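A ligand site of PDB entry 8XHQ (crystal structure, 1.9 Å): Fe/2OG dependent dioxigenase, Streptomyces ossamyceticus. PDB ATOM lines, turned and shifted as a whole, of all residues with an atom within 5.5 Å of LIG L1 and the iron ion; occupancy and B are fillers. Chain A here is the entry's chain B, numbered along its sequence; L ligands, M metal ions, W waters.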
ATOM      1  N   ARG A  83       6.970 -23.258  22.717  1.00  0.00           N
ATOM      2  CA  ARG A  83       7.957 -22.211  22.458  1.00  0.00           C
ATOM      3  C   ARG A  83       7.380 -21.106  21.578  1.00  0.00           C
ATOM      4  O   ARG A  83       6.867 -21.365  20.488  1.00  0.00           O
ATOM      5  CB  ARG A  83       9.200 -22.805  21.805  1.00  0.00           C
ATOM      6  CG  ARG A  83       9.884 -23.776  22.706  1.00  0.00           C
ATOM      7  CD  ARG A  83      10.007 -23.146  24.095  1.00  0.00           C
ATOM      8  NE  ARG A  83      10.896 -23.935  24.881  1.00  0.00           N
ATOM      9  CZ  ARG A  83      11.691 -23.494  25.854  1.00  0.00           C
ATOM     10  NH1 ARG A  83      11.735 -22.206  26.231  1.00  0.00           N
ATOM     11  NH2 ARG A  83      12.437 -24.392  26.458  1.00  0.00           N
ATOM     12  N   HIS A  90       7.756 -29.082  23.186  1.00  0.00           N
ATOM     13  CA  HIS A  90       8.443 -30.262  23.690  1.00  0.00           C
ATOM     14  C   HIS A  90       8.101 -30.531  25.146  1.00  0.00           C
ATOM     15  O   HIS A  90       7.882 -29.615  25.938  1.00  0.00           O
ATOM     16  CB  HIS A  90       9.970 -30.165  23.515  1.00  0.00           C
ATOM     17  CG  HIS A  90      10.569 -28.809  23.797  1.00  0.00           C
ATOM     18  ND1 HIS A  90      11.000 -27.958  22.803  1.00  0.00           N
ATOM     19  CD2 HIS A  90      10.883 -28.186  24.976  1.00  0.00           C
ATOM     20  CE1 HIS A  90      11.525 -26.863  23.336  1.00  0.00           C
ATOM     21  NE2 HIS A  90      11.449 -26.973  24.651  1.00  0.00           N
ATOM     22  N   ILE A  91       8.059 -31.806  25.467  1.00  0.00           N
ATOM     23  CA  ILE A  91       8.161 -32.271  26.837  1.00  0.00           C
ATOM     24  C   ILE A  91       9.613 -32.214  27.266  1.00  0.00           C
ATOM     25  O   ILE A  91      10.508 -32.588  26.505  1.00  0.00           O
ATOM     26  CB  ILE A  91       7.625 -33.710  26.961  1.00  0.00           C
ATOM     27  CG1 ILE A  91       6.122 -33.711  26.710  1.00  0.00           C
ATOM     28  CG2 ILE A  91       7.994 -34.299  28.303  1.00  0.00           C
ATOM     29  CD1 ILE A  91       5.535 -35.091  26.662  1.00  0.00           C
ATOM     30  N   LEU A  92       9.858 -31.764  28.492  1.00  0.00           N
ATOM     31  CA  LEU A  92      11.140 -31.914  29.155  1.00  0.00           C
ATOM     32  C   LEU A  92      10.850 -32.377  30.568  1.00  0.00           C
ATOM     33  O   LEU A  92      10.190 -31.667  31.321  1.00  0.00           O
ATOM     34  CB  LEU A  92      11.952 -30.607  29.161  1.00  0.00           C
ATOM     35  CG  LEU A  92      13.262 -30.761  29.932  1.00  0.00           C
ATOM     36  CD1 LEU A  92      14.327 -31.410  29.059  1.00  0.00           C
ATOM     37  CD2 LEU A  92      13.750 -29.392  30.502  1.00  0.00           C
ATOM     38  N   TRP A 150      17.748 -35.900  32.149  1.00  0.00           N
ATOM     39  CA  TRP A 150      16.645 -35.272  31.424  1.00  0.00           C
ATOM     40  C   TRP A 150      16.175 -36.136  30.256  1.00  0.00           C
ATOM     41  O   TRP A 150      16.941 -36.868  29.630  1.00  0.00           O
ATOM     42  CB  TRP A 150      17.071 -33.918  30.849  1.00  0.00           C
ATOM     43  CG  TRP A 150      17.218 -32.811  31.855  1.00  0.00           C
ATOM     44  CD1 TRP A 150      18.370 -32.141  32.179  1.00  0.00           C
ATOM     45  CD2 TRP A 150      16.178 -32.202  32.630  1.00  0.00           C
ATOM     46  NE1 TRP A 150      18.115 -31.178  33.136  1.00  0.00           N
ATOM     47  CE2 TRP A 150      16.770 -31.184  33.418  1.00  0.00           C
ATOM     48  CE3 TRP A 150      14.801 -32.428  32.752  1.00  0.00           C
ATOM     49  CZ2 TRP A 150      16.035 -30.388  34.311  1.00  0.00           C
ATOM     50  CZ3 TRP A 150      14.063 -31.634  33.636  1.00  0.00           C
ATOM     51  CH2 TRP A 150      14.685 -30.639  34.406  1.00  0.00           C
ATOM     52  N   ALA A 152      13.734 -35.387  26.661  1.00  0.00           N
ATOM     53  CA  ALA A 152      12.980 -34.440  25.850  1.00  0.00           C
ATOM     54  C   ALA A 152      12.238 -35.192  24.745  1.00  0.00           C
ATOM     55  O   ALA A 152      12.788 -36.108  24.121  1.00  0.00           O
ATOM     56  CB  ALA A 152      13.875 -33.367  25.225  1.00  0.00           C
ATOM     57  N   SER A 154      10.247 -33.871  21.314  1.00  0.00           N
ATOM     58  CA  SER A 154       9.993 -32.664  20.527  1.00  0.00           C
ATOM     59  C   SER A 154       9.078 -32.938  19.347  1.00  0.00           C
ATOM     60  O   SER A 154       9.279 -33.920  18.613  1.00  0.00           O
ATOM     61  CB  SER A 154      11.309 -32.061  20.031  1.00  0.00           C
ATOM     62  OG  SER A 154      12.064 -31.572  21.117  1.00  0.00           O
ATOM     63  N   CYS A 165      14.201 -25.272  15.726  1.00  0.00           N
ATOM     64  CA  CYS A 165      14.726 -25.271  17.094  1.00  0.00           C
ATOM     65  C   CYS A 165      15.755 -24.157  17.215  1.00  0.00           C
ATOM     66  O   CYS A 165      16.588 -24.000  16.325  1.00  0.00           O
ATOM     67  CB  CYS A 165      15.399 -26.621  17.446  1.00  0.00           C
ATOM     68  SG  CYS A 165      15.900 -26.841  19.160  1.00  0.00           S
ATOM     69  N   HIS A 168      21.574 -23.913  19.659  1.00  0.00           N
ATOM     70  CA  HIS A 168      22.037 -24.040  21.043  1.00  0.00           C
ATOM     71  C   HIS A 168      23.170 -25.040  21.121  1.00  0.00           C
ATOM     72  O   HIS A 168      23.380 -25.860  20.223  1.00  0.00           O
ATOM     73  CB  HIS A 168      20.904 -24.473  21.985  1.00  0.00           C
ATOM     74  CG  HIS A 168      20.315 -25.806  21.633  1.00  0.00           C
ATOM     75  ND1 HIS A 168      19.406 -25.969  20.617  1.00  0.00           N
ATOM     76  CD2 HIS A 168      20.512 -27.034  22.167  1.00  0.00           C
ATOM     77  CE1 HIS A 168      19.066 -27.236  20.525  1.00  0.00           C
ATOM     78  NE2 HIS A 168      19.713 -27.900  21.468  1.00  0.00           N
ATOM     79  N   LYS A 169      23.890 -24.961  22.233  1.00  0.00           N
ATOM     80  CA  LYS A 169      24.682 -26.063  22.744  1.00  0.00           C
ATOM     81  C   LYS A 169      23.908 -26.737  23.858  1.00  0.00           C
ATOM     82  O   LYS A 169      23.350 -26.072  24.722  1.00  0.00           O
ATOM     83  CB  LYS A 169      26.043 -25.585  23.272  1.00  0.00           C
ATOM     84  CG  LYS A 169      26.893 -24.833  22.218  1.00  0.00           C
ATOM     85  CD  LYS A 169      28.251 -24.385  22.846  1.00  0.00           C
ATOM     86  CE  LYS A 169      29.161 -23.683  21.833  1.00  0.00           C
ATOM     87  NZ  LYS A 169      30.485 -23.300  22.460  1.00  0.00           N
ATOM     88  N   ASP A 170      23.845 -28.068  23.822  1.00  0.00           N
ATOM     89  CA  ASP A 170      23.242 -28.789  24.939  1.00  0.00           C
ATOM     90  C   ASP A 170      23.967 -28.394  26.227  1.00  0.00           C
ATOM     91  O   ASP A 170      25.115 -27.956  26.193  1.00  0.00           O
ATOM     92  CB  ASP A 170      23.320 -30.313  24.704  1.00  0.00           C
ATOM     93  CG  ASP A 170      22.381 -30.752  23.566  1.00  0.00           C
ATOM     94  OD1 ASP A 170      21.530 -29.940  23.199  1.00  0.00           O
ATOM     95  OD2 ASP A 170      22.503 -31.861  23.056  1.00  0.00           O
ATOM     96  N   THR A 171      23.271 -28.487  27.371  1.00  0.00           N
ATOM     97  CA  THR A 171      23.818 -27.879  28.582  1.00  0.00           C
ATOM     98  C   THR A 171      24.579 -28.856  29.458  1.00  0.00           C
ATOM     99  O   THR A 171      25.319 -28.410  30.342  1.00  0.00           O
ATOM    100  CB  THR A 171      22.729 -27.235  29.453  1.00  0.00           C
ATOM    101  OG1 THR A 171      21.718 -28.201  29.762  1.00  0.00           O
ATOM    102  CG2 THR A 171      22.124 -26.046  28.762  1.00  0.00           C
ATOM    103  N   GLY A 172      24.399 -30.157  29.276  1.00  0.00           N
ATOM    104  CA  GLY A 172      24.894 -31.178  30.192  1.00  0.00           C
ATOM    105  C   GLY A 172      26.201 -31.785  29.743  1.00  0.00           C
ATOM    106  O   GLY A 172      27.048 -31.119  29.138  1.00  0.00           O
ATOM    107  N   THR A 175      24.560 -36.211  25.438  1.00  0.00           N
ATOM    108  CA  THR A 175      23.223 -36.323  24.862  1.00  0.00           C
ATOM    109  C   THR A 175      23.141 -37.593  24.016  1.00  0.00           C
ATOM    110  O   THR A 175      24.064 -37.888  23.257  1.00  0.00           O
ATOM    111  CB  THR A 175      22.917 -35.117  23.964  1.00  0.00           C
ATOM    112  OG1 THR A 175      23.093 -33.899  24.700  1.00  0.00           O
ATOM    113  CG2 THR A 175      21.489 -35.213  23.394  1.00  0.00           C
ATOM    114  N   HIS A 226      24.170 -26.444  17.424  1.00  0.00           N
ATOM    115  CA  HIS A 226      23.287 -27.099  16.478  1.00  0.00           C
ATOM    116  C   HIS A 226      21.914 -26.467  16.542  1.00  0.00           C
ATOM    117  O   HIS A 226      21.517 -25.858  17.541  1.00  0.00           O
ATOM    118  CB  HIS A 226      23.211 -28.613  16.738  1.00  0.00           C
ATOM    119  CG  HIS A 226      22.845 -28.972  18.140  1.00  0.00           C
ATOM    120  ND1 HIS A 226      23.733 -28.868  19.194  1.00  0.00           N
ATOM    121  CD2 HIS A 226      21.697 -29.457  18.659  1.00  0.00           C
ATOM    122  CE1 HIS A 226      23.132 -29.261  20.306  1.00  0.00           C
ATOM    123  NE2 HIS A 226      21.902 -29.636  20.008  1.00  0.00           N
ATOM    124  N   PHE A 246      19.542 -36.809  28.334  1.00  0.00           N
ATOM    125  CA  PHE A 246      20.705 -35.973  28.610  1.00  0.00           C
ATOM    126  C   PHE A 246      21.153 -36.244  30.041  1.00  0.00           C
ATOM    127  O   PHE A 246      20.333 -36.259  30.960  1.00  0.00           O
ATOM    128  CB  PHE A 246      20.417 -34.468  28.471  1.00  0.00           C
ATOM    129  CG  PHE A 246      19.566 -34.071  27.282  1.00  0.00           C
ATOM    130  CD1 PHE A 246      18.191 -34.260  27.292  1.00  0.00           C
ATOM    131  CD2 PHE A 246      20.129 -33.403  26.207  1.00  0.00           C
ATOM    132  CE1 PHE A 246      17.416 -33.858  26.215  1.00  0.00           C
ATOM    133  CE2 PHE A 246      19.366 -32.995  25.125  1.00  0.00           C
ATOM    134  CZ  PHE A 246      18.002 -33.219  25.137  1.00  0.00           C
ATOM    135  N   ASN A 248      22.968 -34.571  32.916  1.00  0.00           N
ATOM    136  CA  ASN A 248      23.288 -33.213  33.331  1.00  0.00           C
ATOM    137  C   ASN A 248      23.757 -33.155  34.783  1.00  0.00           C
ATOM    138  O   ASN A 248      23.335 -33.973  35.610  1.00  0.00           O
ATOM    139  CB  ASN A 248      22.070 -32.273  33.215  1.00  0.00           C
ATOM    140  CG  ASN A 248      21.958 -31.630  31.866  1.00  0.00           C
ATOM    141  OD1 ASN A 248      21.998 -30.393  31.742  1.00  0.00           O
ATOM    142  ND2 ASN A 248      21.805 -32.452  30.843  1.00  0.00           N
ATOM    143  N   LEU A 274      22.516 -22.141  33.582  1.00  0.00           N
ATOM    144  CA  LEU A 274      21.293 -22.517  32.878  1.00  0.00           C
ATOM    145  C   LEU A 274      20.409 -21.303  32.604  1.00  0.00           C
ATOM    146  O   LEU A 274      19.761 -21.210  31.540  1.00  0.00           O
ATOM    147  CB  LEU A 274      20.524 -23.571  33.693  1.00  0.00           C
ATOM    148  CG  LEU A 274      21.217 -24.930  33.849  1.00  0.00           C
ATOM    149  CD1 LEU A 274      20.476 -25.807  34.863  1.00  0.00           C
ATOM    150  CD2 LEU A 274      21.303 -25.650  32.500  1.00  0.00           C
ATOM    151  N   PHE A 277      21.846 -19.555  29.763  1.00  0.00           N
ATOM    152  CA  PHE A 277      21.471 -20.378  28.611  1.00  0.00           C
ATOM    153  C   PHE A 277      20.036 -20.091  28.170  1.00  0.00           C
ATOM    154  O   PHE A 277      19.776 -19.857  26.991  1.00  0.00           O
ATOM    155  CB  PHE A 277      21.652 -21.864  28.932  1.00  0.00           C
ATOM    156  CG  PHE A 277      21.115 -22.773  27.855  1.00  0.00           C
ATOM    157  CD1 PHE A 277      19.777 -23.183  27.874  1.00  0.00           C
ATOM    158  CD2 PHE A 277      21.927 -23.198  26.821  1.00  0.00           C
ATOM    159  CE1 PHE A 277      19.265 -24.018  26.875  1.00  0.00           C
ATOM    160  CE2 PHE A 277      21.425 -24.035  25.819  1.00  0.00           C
ATOM    161  CZ  PHE A 277      20.099 -24.447  25.845  1.00  0.00           C
ATOM    162  N   ASN A 278      19.067 -20.168  29.104  1.00  0.00           N
ATOM    163  CA  ASN A 278      17.678 -19.946  28.710  1.00  0.00           C
ATOM    164  C   ASN A 278      17.479 -18.549  28.122  1.00  0.00           C
ATOM    165  O   ASN A 278      16.742 -18.378  27.150  1.00  0.00           O
ATOM    166  CB  ASN A 278      16.732 -20.153  29.888  1.00  0.00           C
ATOM    167  CG  ASN A 278      16.611 -21.616  30.315  1.00  0.00           C
ATOM    168  OD1 ASN A 278      16.993 -22.512  29.573  1.00  0.00           O
ATOM    169  ND2 ASN A 278      16.086 -21.852  31.508  1.00  0.00           N
ATOM    170  N   THR A 281      19.117 -18.454  24.546  1.00  0.00           N
ATOM    171  CA  THR A 281      18.677 -19.476  23.602  1.00  0.00           C
ATOM    172  C   THR A 281      17.197 -19.319  23.280  1.00  0.00           C
ATOM    173  O   THR A 281      16.807 -19.217  22.108  1.00  0.00           O
ATOM    174  CB  THR A 281      18.923 -20.879  24.176  1.00  0.00           C
ATOM    175  OG1 THR A 281      20.304 -21.055  24.481  1.00  0.00           O
ATOM    176  CG2 THR A 281      18.485 -21.947  23.175  1.00  0.00           C
ATOM    177  N   TRP A 282      16.357 -19.347  24.302  1.00  0.00           N
ATOM    178  CA  TRP A 282      14.914 -19.319  24.113  1.00  0.00           C
ATOM    179  C   TRP A 282      14.343 -17.932  24.316  1.00  0.00           C
ATOM    180  O   TRP A 282      13.539 -17.473  23.496  1.00  0.00           O
ATOM    181  CB  TRP A 282      14.247 -20.316  25.066  1.00  0.00           C
ATOM    182  CG  TRP A 282      14.707 -21.736  24.819  1.00  0.00           C
ATOM    183  CD1 TRP A 282      15.514 -22.488  25.616  1.00  0.00           C
ATOM    184  CD2 TRP A 282      14.428 -22.533  23.664  1.00  0.00           C
ATOM    185  NE1 TRP A 282      15.742 -23.716  25.046  1.00  0.00           N
ATOM    186  CE2 TRP A 282      15.082 -23.768  23.847  1.00  0.00           C
ATOM    187  CE3 TRP A 282      13.683 -22.320  22.497  1.00  0.00           C
ATOM    188  CZ2 TRP A 282      15.002 -24.795  22.903  1.00  0.00           C
ATOM    189  CZ3 TRP A 282      13.612 -23.349  21.551  1.00  0.00           C
ATOM    190  CH2 TRP A 282      14.260 -24.565  21.765  1.00  0.00           C
ATOM    191  N   PHE A 289      12.940 -23.325  32.746  1.00  0.00           N
ATOM    192  CA  PHE A 289      13.061 -24.514  31.898  1.00  0.00           C
ATOM    193  C   PHE A 289      14.378 -25.232  32.173  1.00  0.00           C
ATOM    194  O   PHE A 289      15.457 -24.635  32.053  1.00  0.00           O
ATOM    195  CB  PHE A 289      12.961 -24.084  30.426  1.00  0.00           C
ATOM    196  CG  PHE A 289      13.257 -25.176  29.421  1.00  0.00           C
ATOM    197  CD1 PHE A 289      12.291 -26.131  29.097  1.00  0.00           C
ATOM    198  CD2 PHE A 289      14.483 -25.188  28.735  1.00  0.00           C
ATOM    199  CE1 PHE A 289      12.557 -27.129  28.143  1.00  0.00           C
ATOM    200  CE2 PHE A 289      14.748 -26.186  27.780  1.00  0.00           C
ATOM    201  CZ  PHE A 289      13.781 -27.152  27.501  1.00  0.00           C
ATOM    202  N   GLY A 290      14.291 -26.508  32.530  1.00  0.00           N
ATOM    203  CA  GLY A 290      15.509 -27.253  32.799  1.00  0.00           C
ATOM    204  C   GLY A 290      16.169 -26.949  34.121  1.00  0.00           C
ATOM    205  O   GLY A 290      17.302 -27.371  34.351  1.00  0.00           O
HETATM  206  C1  LIG L   1      18.993 -28.620  27.529  1.00  0.00           C
HETATM  207  C2  LIG L   1      19.671 -29.365  26.371  1.00  0.00           C
HETATM  208  C3  LIG L   1      17.904 -28.474  24.743  1.00  0.00           C
HETATM  209  C4  LIG L   1      17.738 -27.306  25.726  1.00  0.00           C
HETATM  210  C5  LIG L   1      17.984 -29.517  28.272  1.00  0.00           C
HETATM  211  C6  LIG L   1      18.648 -30.804  28.746  1.00  0.00           C
HETATM  212  C7  LIG L   1      17.452 -28.713  29.490  1.00  0.00           C
HETATM  213  C8  LIG L   1      18.563 -28.315  30.472  1.00  0.00           C
HETATM  214  C9  LIG L   1      16.641 -29.370  24.731  1.00  0.00           C
HETATM  215  C10 LIG L   1      15.460 -28.655  24.009  1.00  0.00           C
HETATM  216  C11 LIG L   1      14.257 -29.613  24.167  1.00  0.00           C
HETATM  217  C12 LIG L   1      15.750 -28.445  22.515  1.00  0.00           C
HETATM  218  N1  LIG L   1      18.288 -27.410  27.079  1.00  0.00           N
HETATM  219  N2  LIG L   1      19.098 -29.273  25.027  1.00  0.00           N
HETATM  220  O1  LIG L   1      17.172 -26.299  25.398  1.00  0.00           O
HETATM  221  O2  LIG L   1      20.655 -30.014  26.543  1.00  0.00           O
HETATM  222  O3  LIG L   1      19.183 -27.097  30.097  1.00  0.00           O
HETATM  223  C1  LG2 L   2      17.646 -31.342  21.708  1.00  0.00           C
HETATM  224  O1  LG2 L   2      18.404 -30.780  22.516  1.00  0.00           O
HETATM  225  O2  LG2 L   2      16.679 -32.017  22.130  1.00  0.00           O
HETATM  226  C2  LG2 L   2      17.851 -31.193  20.260  1.00  0.00           C
HETATM  227  O3  LG2 L   2      18.748 -30.529  19.798  1.00  0.00           O
HETATM  228  C3  LG2 L   2      16.978 -31.896  19.255  1.00  0.00           C
HETATM  229  C4  LG2 L   2      17.501 -31.607  17.832  1.00  0.00           C
HETATM  230  C5  LG2 L   2      16.590 -32.338  16.843  1.00  0.00           C
HETATM  231  O4  LG2 L   2      17.100 -32.946  15.891  1.00  0.00           O
HETATM  232  O5  LG2 L   2      15.345 -32.305  17.002  1.00  0.00           O
HETATM  233 FE    FE M   1      20.236 -30.082  21.403  1.00  0.00          FE
HETATM  234  O   HOH W   1      17.780 -25.040  30.765  1.00  0.00           O
HETATM  235  O   HOH W   2      22.269 -31.557  28.112  1.00  0.00           O
HETATM  236  O   HOH W   3      20.826 -32.294  21.108  1.00  0.00           O
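N2 of LIG L1 lies close to OD1 of Asp 170 (3.1 Å).
An oxygen (O2) of LIG L1 is in hydrogen-bond range of the backbone NH (N) of Thr 171.
OG1 of Thr 171 is in hydrogen-bond range of O3 of LIG L1, at 2.8 Å.
The indole nitrogen (NE1) of Trp 282 is in hydrogen-bond range of an oxygen (O1) of LIG L1, at 3.0 Å.
N2 of LIG L1 sits close to O1 of LG2 L2.
OD2 of Asp 170 sits at hydrogen-bond distance from OG1 of Thr 175 (2.7 Å).
The side-chain hydroxyl (OG1) of Thr 171 is in hydrogen-bond range of the side-chain amide oxygen (OD1) of Asn 248.
The backbone carbonyl oxygen (O) of Phe 289 lies within hydrogen-bond range of the side-chain amide nitrogen (ND2) of Asn 278, 2.9 Å away.
The backbone carbonyl oxygen of Phe 277 is in hydrogen-bond range of the side-chain hydroxyl of Thr 281 (2.8 Å).
The backbone NH of Trp 150 sits at hydrogen-bond distance from the backbone carbonyl oxygen of Phe 246 (2.9 Å).
A ring nitrogen (NE2) of His 90 is in hydrogen-bond range of the guanidinium group (NE) of Arg 83 (3.1 Å).
His 90 touches LIG L1 (CD2 to C11, 3.8 Å).
Leu 92 touches LIG L1 (CD2 to C7, 3.9 Å).
Trp 150 touches LIG L1 (CD1 to C6, 3.7 Å).
Ala 152 touches LIG L1.
Cys 165 touches LIG L1.
Phe 246 touches LIG L1.
CD2 of Leu 274 touches O3 of LIG L1, at 3.5 Å.
Phe 277 touches LIG L1 (CE1 to O1, 3.4 Å).
Phe 289 touches LIG L1 (CE2 to O1, 3.4 Å).
CA of Gly 290 touches C8 of LIG L1 (3.98 Å).
Within 4 Å of LIG L1: His 90, Leu 92, Trp 150, Ala 152, Cys 165, His 168, Asp 170, Thr 171, Phe 246, Leu 274, Phe 277, Trp 282, Phe 289 and Gly 290.
The nearest printed residue that does not touch LIG L1 is Asn 248 (4.1 Å).
The iron ion is bound by a ring nitrogen (NE2) of His 226 (2.2 Å), the side-chain carboxylate (OD1) of Asp 170 (2.2 Å), an oxygen (O3) of LG2 L2 (2.2 Å), a ring nitrogen (NE2) of His 168 (2.2 Å), an oxygen (O1) of LG2 L2 (2.3 Å) and water W3 (2.3 Å).
Water W1 lies within hydrogen-bond range of O3 of LIG L1, O of Phe 289 and OD1 of Asn 278.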
